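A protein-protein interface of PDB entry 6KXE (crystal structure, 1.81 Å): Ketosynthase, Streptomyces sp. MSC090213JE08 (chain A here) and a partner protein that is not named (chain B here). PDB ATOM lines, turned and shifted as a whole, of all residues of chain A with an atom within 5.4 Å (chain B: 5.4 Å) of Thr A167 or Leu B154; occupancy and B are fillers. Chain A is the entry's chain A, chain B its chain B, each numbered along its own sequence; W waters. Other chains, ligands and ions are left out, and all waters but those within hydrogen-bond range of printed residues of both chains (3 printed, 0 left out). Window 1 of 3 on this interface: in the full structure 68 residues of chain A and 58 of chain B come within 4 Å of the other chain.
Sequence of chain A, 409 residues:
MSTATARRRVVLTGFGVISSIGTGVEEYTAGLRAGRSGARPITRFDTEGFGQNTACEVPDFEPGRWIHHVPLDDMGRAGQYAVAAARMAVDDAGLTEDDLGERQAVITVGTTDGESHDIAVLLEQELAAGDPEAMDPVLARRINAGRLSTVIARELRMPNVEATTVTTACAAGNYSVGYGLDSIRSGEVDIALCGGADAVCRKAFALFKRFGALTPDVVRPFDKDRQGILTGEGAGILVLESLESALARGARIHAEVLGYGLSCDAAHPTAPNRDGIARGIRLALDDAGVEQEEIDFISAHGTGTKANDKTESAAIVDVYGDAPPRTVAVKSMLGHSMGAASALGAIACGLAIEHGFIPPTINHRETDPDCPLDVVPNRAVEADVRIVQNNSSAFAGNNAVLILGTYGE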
ATOM      1  N   THR A 111     -24.963  32.169  -9.238  1.00  0.00           N
ATOM      2  CA  THR A 111     -25.900  31.022  -9.112  1.00  0.00           C
ATOM      3  C   THR A 111     -25.163  29.700  -9.372  1.00  0.00           C
ATOM      4  O   THR A 111     -24.226  29.634 -10.210  1.00  0.00           O
ATOM      5  CB  THR A 111     -27.132  31.226 -10.002  1.00  0.00           C
ATOM      6  OG1 THR A 111     -28.144  30.289  -9.629  1.00  0.00           O
ATOM      7  CG2 THR A 111     -26.838  30.995 -11.467  1.00  0.00           C
ATOM      8  N   THR A 112     -25.642  28.639  -8.747  1.00  0.00           N
ATOM      9  CA  THR A 112     -25.187  27.267  -9.004  1.00  0.00           C
ATOM     10  C   THR A 112     -26.112  26.621 -10.044  1.00  0.00           C
ATOM     11  O   THR A 112     -25.604  26.060 -11.016  1.00  0.00           O
ATOM     12  CB  THR A 112     -25.158  26.426  -7.728  1.00  0.00           C
ATOM     13  OG1 THR A 112     -24.198  26.976  -6.825  1.00  0.00           O
ATOM     14  CG2 THR A 112     -24.818  24.972  -8.006  1.00  0.00           C
ATOM     15  N   ASP A 113     -27.416  26.655  -9.813  1.00  0.00           N
ATOM     16  CA  ASP A 113     -28.424  25.860 -10.552  1.00  0.00           C
ATOM     17  C   ASP A 113     -29.404  26.750 -11.325  1.00  0.00           C
ATOM     18  O   ASP A 113     -30.103  26.208 -12.199  1.00  0.00           O
ATOM     19  CB  ASP A 113     -29.191  24.965  -9.578  1.00  0.00           C
ATOM     20  CG  ASP A 113     -28.330  23.935  -8.895  1.00  0.00           C
ATOM     21  OD1 ASP A 113     -27.572  23.248  -9.611  1.00  0.00           O
ATOM     22  OD2 ASP A 113     -28.353  23.896  -7.655  1.00  0.00           O
ATOM     23  N   ALA A 145     -29.214  31.291 -17.229  1.00  0.00           N
ATOM     24  CA  ALA A 145     -28.699  31.922 -15.992  1.00  0.00           C
ATOM     25  C   ALA A 145     -28.511  33.423 -16.181  1.00  0.00           C
ATOM     26  O   ALA A 145     -28.636  34.183 -15.171  1.00  0.00           O
ATOM     27  CB  ALA A 145     -27.429  31.254 -15.536  1.00  0.00           C
ATOM     28  N   THR A 165     -24.278  37.325 -14.842  1.00  0.00           N
ATOM     29  CA  THR A 165     -24.495  36.197 -13.932  1.00  0.00           C
ATOM     30  C   THR A 165     -23.206  35.379 -13.846  1.00  0.00           C
ATOM     31  O   THR A 165     -22.716  34.901 -14.885  1.00  0.00           O
ATOM     32  CB  THR A 165     -25.670  35.342 -14.389  1.00  0.00           C
ATOM     33  OG1 THR A 165     -26.853  36.147 -14.423  1.00  0.00           O
ATOM     34  CG2 THR A 165     -25.869  34.161 -13.465  1.00  0.00           C
ATOM     35  N   VAL A 166     -22.662  35.249 -12.648  1.00  0.00           N
ATOM     36  CA  VAL A 166     -21.430  34.464 -12.387  1.00  0.00           C
ATOM     37  C   VAL A 166     -21.831  33.038 -11.995  1.00  0.00           C
ATOM     38  O   VAL A 166     -22.526  32.863 -10.989  1.00  0.00           O
ATOM     39  CB  VAL A 166     -20.566  35.141 -11.315  1.00  0.00           C
ATOM     40  CG1 VAL A 166     -19.387  34.257 -10.974  1.00  0.00           C
ATOM     41  CG2 VAL A 166     -20.099  36.499 -11.800  1.00  0.00           C
ATOM     42  N   THR A 167     -21.433  32.056 -12.795  1.00  0.00           N
ATOM     43  CA  THR A 167     -21.776  30.616 -12.619  1.00  0.00           C
ATOM     44  C   THR A 167     -20.525  29.894 -12.095  1.00  0.00           C
ATOM     45  O   THR A 167     -20.011  29.011 -12.776  1.00  0.00           O
ATOM     46  CB  THR A 167     -22.410  30.082 -13.911  1.00  0.00           C
ATOM     47  OG1 THR A 167     -21.438  30.195 -14.947  1.00  0.00           O
ATOM     48  CG2 THR A 167     -23.638  30.845 -14.326  1.00  0.00           C
ATOM     49  N   THR A 168     -20.082  30.233 -10.879  1.00  0.00           N
ATOM     50  CA  THR A 168     -18.969  29.524 -10.201  1.00  0.00           C
ATOM     51  C   THR A 168     -19.552  28.766  -9.003  1.00  0.00           C
ATOM     52  O   THR A 168     -18.927  28.745  -7.915  1.00  0.00           O
ATOM     53  CB  THR A 168     -17.860  30.504  -9.836  1.00  0.00           C
ATOM     54  OG1 THR A 168     -18.426  31.573  -9.070  1.00  0.00           O
ATOM     55  CG2 THR A 168     -17.173  31.077 -11.063  1.00  0.00           C
ATOM     56  N   ALA A 169     -20.759  28.227  -9.193  1.00  0.00           N
ATOM     57  CA  ALA A 169     -21.382  27.223  -8.312  1.00  0.00           C
ATOM     58  C   ALA A 169     -21.343  27.740  -6.858  1.00  0.00           C
ATOM     59  O   ALA A 169     -21.807  28.892  -6.614  1.00  0.00           O
ATOM     60  CB  ALA A 169     -20.617  25.937  -8.540  1.00  0.00           C
ATOM     61  N   ALA A 172     -20.210  31.419  -5.941  1.00  0.00           N
ATOM     62  CA  ALA A 172     -20.662  32.427  -6.920  1.00  0.00           C
ATOM     63  C   ALA A 172     -20.941  33.776  -6.230  1.00  0.00           C
ATOM     64  O   ALA A 172     -20.477  34.796  -6.742  1.00  0.00           O
ATOM     65  CB  ALA A 172     -21.819  31.881  -7.687  1.00  0.00           C
ATOM     66  N   ASN A 398     -12.888  26.038  -7.630  1.00  0.00           N
ATOM     67  CA  ASN A 398     -13.044  27.507  -7.615  1.00  0.00           C
ATOM     68  C   ASN A 398     -13.107  27.961  -6.156  1.00  0.00           C
ATOM     69  O   ASN A 398     -14.035  27.520  -5.396  1.00  0.00           O
ATOM     70  CB  ASN A 398     -14.287  27.943  -8.396  1.00  0.00           C
ATOM     71  CG  ASN A 398     -14.216  27.881  -9.915  1.00  0.00           C
ATOM     72  OD1 ASN A 398     -15.188  28.282 -10.561  1.00  0.00           O
ATOM     73  ND2 ASN A 398     -13.131  27.392 -10.507  1.00  0.00           N
ATOM     74  N   ILE B 120     -20.867  31.235 -21.061  1.00  0.00           N
ATOM     75  CA  ILE B 120     -21.806  30.138 -21.425  1.00  0.00           C
ATOM     76  C   ILE B 120     -23.224  30.698 -21.558  1.00  0.00           C
ATOM     77  O   ILE B 120     -23.459  31.880 -21.227  1.00  0.00           O
ATOM     78  CB  ILE B 120     -21.780  29.009 -20.373  1.00  0.00           C
ATOM     79  CG1 ILE B 120     -22.122  29.545 -18.980  1.00  0.00           C
ATOM     80  CG2 ILE B 120     -20.455  28.274 -20.413  1.00  0.00           C
ATOM     81  CD1 ILE B 120     -22.311  28.443 -17.909  1.00  0.00           C
ATOM     82  N   MET B 122     -26.028  28.111 -20.554  1.00  0.00           N
ATOM     83  CA  MET B 122     -26.596  27.368 -19.409  1.00  0.00           C
ATOM     84  C   MET B 122     -25.839  26.034 -19.282  1.00  0.00           C
ATOM     85  O   MET B 122     -26.416  25.035 -18.832  1.00  0.00           O
ATOM     86  CB  MET B 122     -28.110  27.205 -19.574  1.00  0.00           C
ATOM     87  CG  MET B 122     -28.808  26.768 -18.265  1.00  0.00           C
ATOM     88  SD  MET B 122     -28.394  27.851 -16.922  1.00  0.00           S
ATOM     89  CE  MET B 122     -29.388  27.142 -15.598  1.00  0.00           C
ATOM     90  N   GLY B 123     -24.549  26.051 -19.653  1.00  0.00           N
ATOM     91  CA  GLY B 123     -23.654  24.891 -19.551  1.00  0.00           C
ATOM     92  C   GLY B 123     -24.102  23.775 -20.483  1.00  0.00           C
ATOM     93  O   GLY B 123     -24.664  24.058 -21.610  1.00  0.00           O
ATOM     94  N   SER B 124     -23.920  22.541 -20.022  1.00  0.00           N
ATOM     95  CA  SER B 124     -24.342  21.332 -20.773  1.00  0.00           C
ATOM     96  C   SER B 124     -25.789  21.006 -20.406  1.00  0.00           C
ATOM     97  O   SER B 124     -26.027  20.393 -19.343  1.00  0.00           O
ATOM     98  CB  SER B 124     -23.430  20.169 -20.506  1.00  0.00           C
ATOM     99  OG  SER B 124     -23.922  19.025 -21.221  1.00  0.00           O
ATOM    100  N   GLY B 152     -21.484  18.133 -14.797  1.00  0.00           N
ATOM    101  CA  GLY B 152     -22.720  18.929 -14.811  1.00  0.00           C
ATOM    102  C   GLY B 152     -22.518  20.372 -14.364  1.00  0.00           C
ATOM    103  O   GLY B 152     -23.323  21.215 -14.789  1.00  0.00           O
ATOM    104  N   SER B 153     -21.573  20.644 -13.465  1.00  0.00           N
ATOM    105  CA  SER B 153     -21.369  22.000 -12.895  1.00  0.00           C
ATOM    106  C   SER B 153     -21.175  23.021 -14.043  1.00  0.00           C
ATOM    107  O   SER B 153     -20.422  22.713 -15.035  1.00  0.00           O
ATOM    108  CB  SER B 153     -20.218  21.983 -11.913  1.00  0.00           C
ATOM    109  OG  SER B 153     -20.257  23.126 -11.056  1.00  0.00           O
ATOM    110  N   LEU B 154     -21.810  24.190 -13.948  1.00  0.00           N
ATOM    111  CA  LEU B 154     -21.761  25.224 -15.030  1.00  0.00           C
ATOM    112  C   LEU B 154     -20.302  25.695 -15.230  1.00  0.00           C
ATOM    113  O   LEU B 154     -19.925  26.054 -16.348  1.00  0.00           O
ATOM    114  CB  LEU B 154     -22.671  26.407 -14.676  1.00  0.00           C
ATOM    115  CG  LEU B 154     -24.162  26.070 -14.605  1.00  0.00           C
ATOM    116  CD1 LEU B 154     -24.988  27.302 -14.327  1.00  0.00           C
ATOM    117  CD2 LEU B 154     -24.623  25.398 -15.889  1.00  0.00           C
ATOM    118  N   ASN B 155     -19.515  25.665 -14.169  1.00  0.00           N
ATOM    119  CA  ASN B 155     -18.088  26.066 -14.192  1.00  0.00           C
ATOM    120  C   ASN B 155     -17.178  24.889 -14.558  1.00  0.00           C
ATOM    121  O   ASN B 155     -15.993  25.092 -14.512  1.00  0.00           O
ATOM    122  CB  ASN B 155     -17.690  26.721 -12.871  1.00  0.00           C
ATOM    123  CG  ASN B 155     -17.760  25.808 -11.667  1.00  0.00           C
ATOM    124  OD1 ASN B 155     -18.319  24.705 -11.732  1.00  0.00           O
ATOM    125  ND2 ASN B 155     -17.237  26.295 -10.546  1.00  0.00           N
ATOM    126  N   HIS B 156     -17.684  23.735 -15.031  1.00  0.00           N
ATOM    127  CA  HIS B 156     -16.815  22.562 -15.217  1.00  0.00           C
ATOM    128  C   HIS B 156     -15.797  22.833 -16.323  1.00  0.00           C
ATOM    129  O   HIS B 156     -14.621  22.461 -16.125  1.00  0.00           O
ATOM    130  CB  HIS B 156     -17.561  21.264 -15.546  1.00  0.00           C
ATOM    131  CG  HIS B 156     -16.607  20.125 -15.553  1.00  0.00           C
ATOM    132  ND1 HIS B 156     -16.105  19.645 -16.724  1.00  0.00           N
ATOM    133  CD2 HIS B 156     -15.959  19.490 -14.547  1.00  0.00           C
ATOM    134  CE1 HIS B 156     -15.253  18.665 -16.430  1.00  0.00           C
ATOM    135  NE2 HIS B 156     -15.126  18.570 -15.103  1.00  0.00           N
ATOM    136  N   ALA B 157     -16.219  23.417 -17.441  1.00  0.00           N
ATOM    137  CA  ALA B 157     -15.328  23.624 -18.609  1.00  0.00           C
ATOM    138  C   ALA B 157     -14.134  24.498 -18.186  1.00  0.00           C
ATOM    139  O   ALA B 157     -12.979  24.153 -18.502  1.00  0.00           O
ATOM    140  CB  ALA B 157     -16.109  24.190 -19.772  1.00  0.00           C
ATOM    141  N   THR B 173     -16.480  31.495 -14.562  1.00  0.00           N
ATOM    142  CA  THR B 173     -17.455  31.246 -15.649  1.00  0.00           C
ATOM    143  C   THR B 173     -18.565  32.270 -15.521  1.00  0.00           C
ATOM    144  O   THR B 173     -19.034  32.521 -14.371  1.00  0.00           O
ATOM    145  CB  THR B 173     -17.971  29.809 -15.591  1.00  0.00           C
ATOM    146  OG1 THR B 173     -16.880  28.888 -15.589  1.00  0.00           O
ATOM    147  CG2 THR B 173     -18.907  29.472 -16.731  1.00  0.00           C
ATOM    148  N   VAL B 174     -18.979  32.855 -16.654  1.00  0.00           N
ATOM    149  CA  VAL B 174     -20.078  33.849 -16.663  1.00  0.00           C
ATOM    150  C   VAL B 174     -21.107  33.387 -17.674  1.00  0.00           C
ATOM    151  O   VAL B 174     -20.724  32.767 -18.681  1.00  0.00           O
ATOM    152  CB  VAL B 174     -19.588  35.278 -16.942  1.00  0.00           C
ATOM    153  CG1 VAL B 174     -18.629  35.777 -15.888  1.00  0.00           C
ATOM    154  CG2 VAL B 174     -18.976  35.418 -18.333  1.00  0.00           C
ATOM    155  N   ALA B 175     -22.383  33.647 -17.390  1.00  0.00           N
ATOM    156  CA  ALA B 175     -23.468  33.332 -18.339  1.00  0.00           C
ATOM    157  C   ALA B 175     -23.740  34.556 -19.212  1.00  0.00           C
ATOM    158  O   ALA B 175     -22.916  35.474 -19.268  1.00  0.00           O
ATOM    159  CB  ALA B 175     -24.670  32.818 -17.585  1.00  0.00           C
HETATM  160  O   HOH W   1     -24.644  36.944 -17.603  1.00  0.00           O
HETATM  161  O   HOH W   2     -23.105  24.990 -11.430  1.00  0.00           O
HETATM  162  O   HOH W   3     -15.018  28.845 -13.413  1.00  0.00           O
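O of Thr B173 lies within hydrogen-bond range of N of Thr A167, 2.9 Å away.
The side-chain amide oxygen (OD1) of Asn A398 is in hydrogen-bond range of the side-chain amide nitrogen (ND2) of Asn B155 (2.9 Å).
The backbone NH (N) of Ala B175 is in hydrogen-bond range of the backbone carbonyl oxygen (O) of Thr A165 (2.8 Å).
SD of Met B122 is in hydrogen-bond range of N of Ala A145 (3.5 Å).
Water W2 lies within hydrogen-bond range of O of Thr A112 (2.7 Å), N of Leu B154 (2.9 Å) and OG of Ser B153 (3.4 Å).
Water W1 bridges N of Thr A165 (2.8 Å) and O of Ala B175 (2.8 Å).
Water W3 lies within hydrogen-bond range of the side-chain hydroxyl (OG1) of Thr B173 and the side-chain amide oxygen (OD1) of Asn A398.
O of Ala A145 sits at hydrogen-bond distance from OG1 of Thr A165.
OG of Ser B153 lies within hydrogen-bond range of OD1 of Asn B155, 2.6 Å away.
N of Thr A111 is in hydrogen-bond range of O of Val A166, 3.1 Å away.
The backbone NH of Ile B120 sits at hydrogen-bond distance from the backbone carbonyl oxygen of Val B174, at 2.8 Å.
OG1 of Thr A112 sits close to O of Ala A169, 3.1 Å away.
Leu B154 touches Thr A112.
Asp A113 touches Met B122.
Thr A165 touches Val B174 (O to CA, 3.4 Å).
O of Thr B173 touches CA of Val A166 (3.7 Å).
Leu B154 touches Thr A167 (CB to CB, 3.8 Å).
CB of Asn B155 touches O of Thr A167, 3.3 Å away.
Ala B175 touches Thr A167 (CB to CG2, 3.9 Å).
CA of Thr A168 touches ND2 of Asn B155, 3.7 Å away.
Thr A168 touches Thr B173 (CG2 to N, 3.6 Å).
CB of Ala A169 touches OG of Ser B153, 3.8 Å away.
Printed residues of chain B within 4 Å of Thr A167: Ile B120, Leu B154, Asn B155, Thr B173 and Ala B175.
Of the printed residues of chain B, Ala A169 touches Ser B153 (3.8 Å) and Asn B155 (3.9 Å).
Of the printed residues of chain A, Ile B120 touches Thr A167.
Of the printed residues of chain A, Ala B175 touches Ala A145, Thr A165 and Thr A167.
Of the printed residues of chain B, Thr A168 touches Asn B155 and Thr B173.
Gly B123 touches none of the printed residues of chain A.
The nearest printed residue of chain B that does not touch Thr A167 is Val B174 (4.005 Å).
The nearest printed residue of chain A that does not touch Leu B154 is Thr A111 (4.8 Å).
Printed residues of chain A that touch a printed residue of chain B: Thr A112, Asp A113, Ala A145, Thr A165, Val A166, Thr A167, Thr A168, Ala A169 and Asn A398.
Printed residues of chain B that touch a printed residue of chain A: Ile B120, Met B122, Ser B153, Leu B154, Asn B155, Thr B173, Val B174 and Ala B175.
Hydrophobic or aromatic side chains of chain B that line the printed part of chain A: Ile B120, Met B122, Leu B154, Val B174 and Ala B175.
Along chain B the printed residues that touch a printed residue of chain A span positions 120 to 175.
Among the printed residues, 17 pairs touch across the chains.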
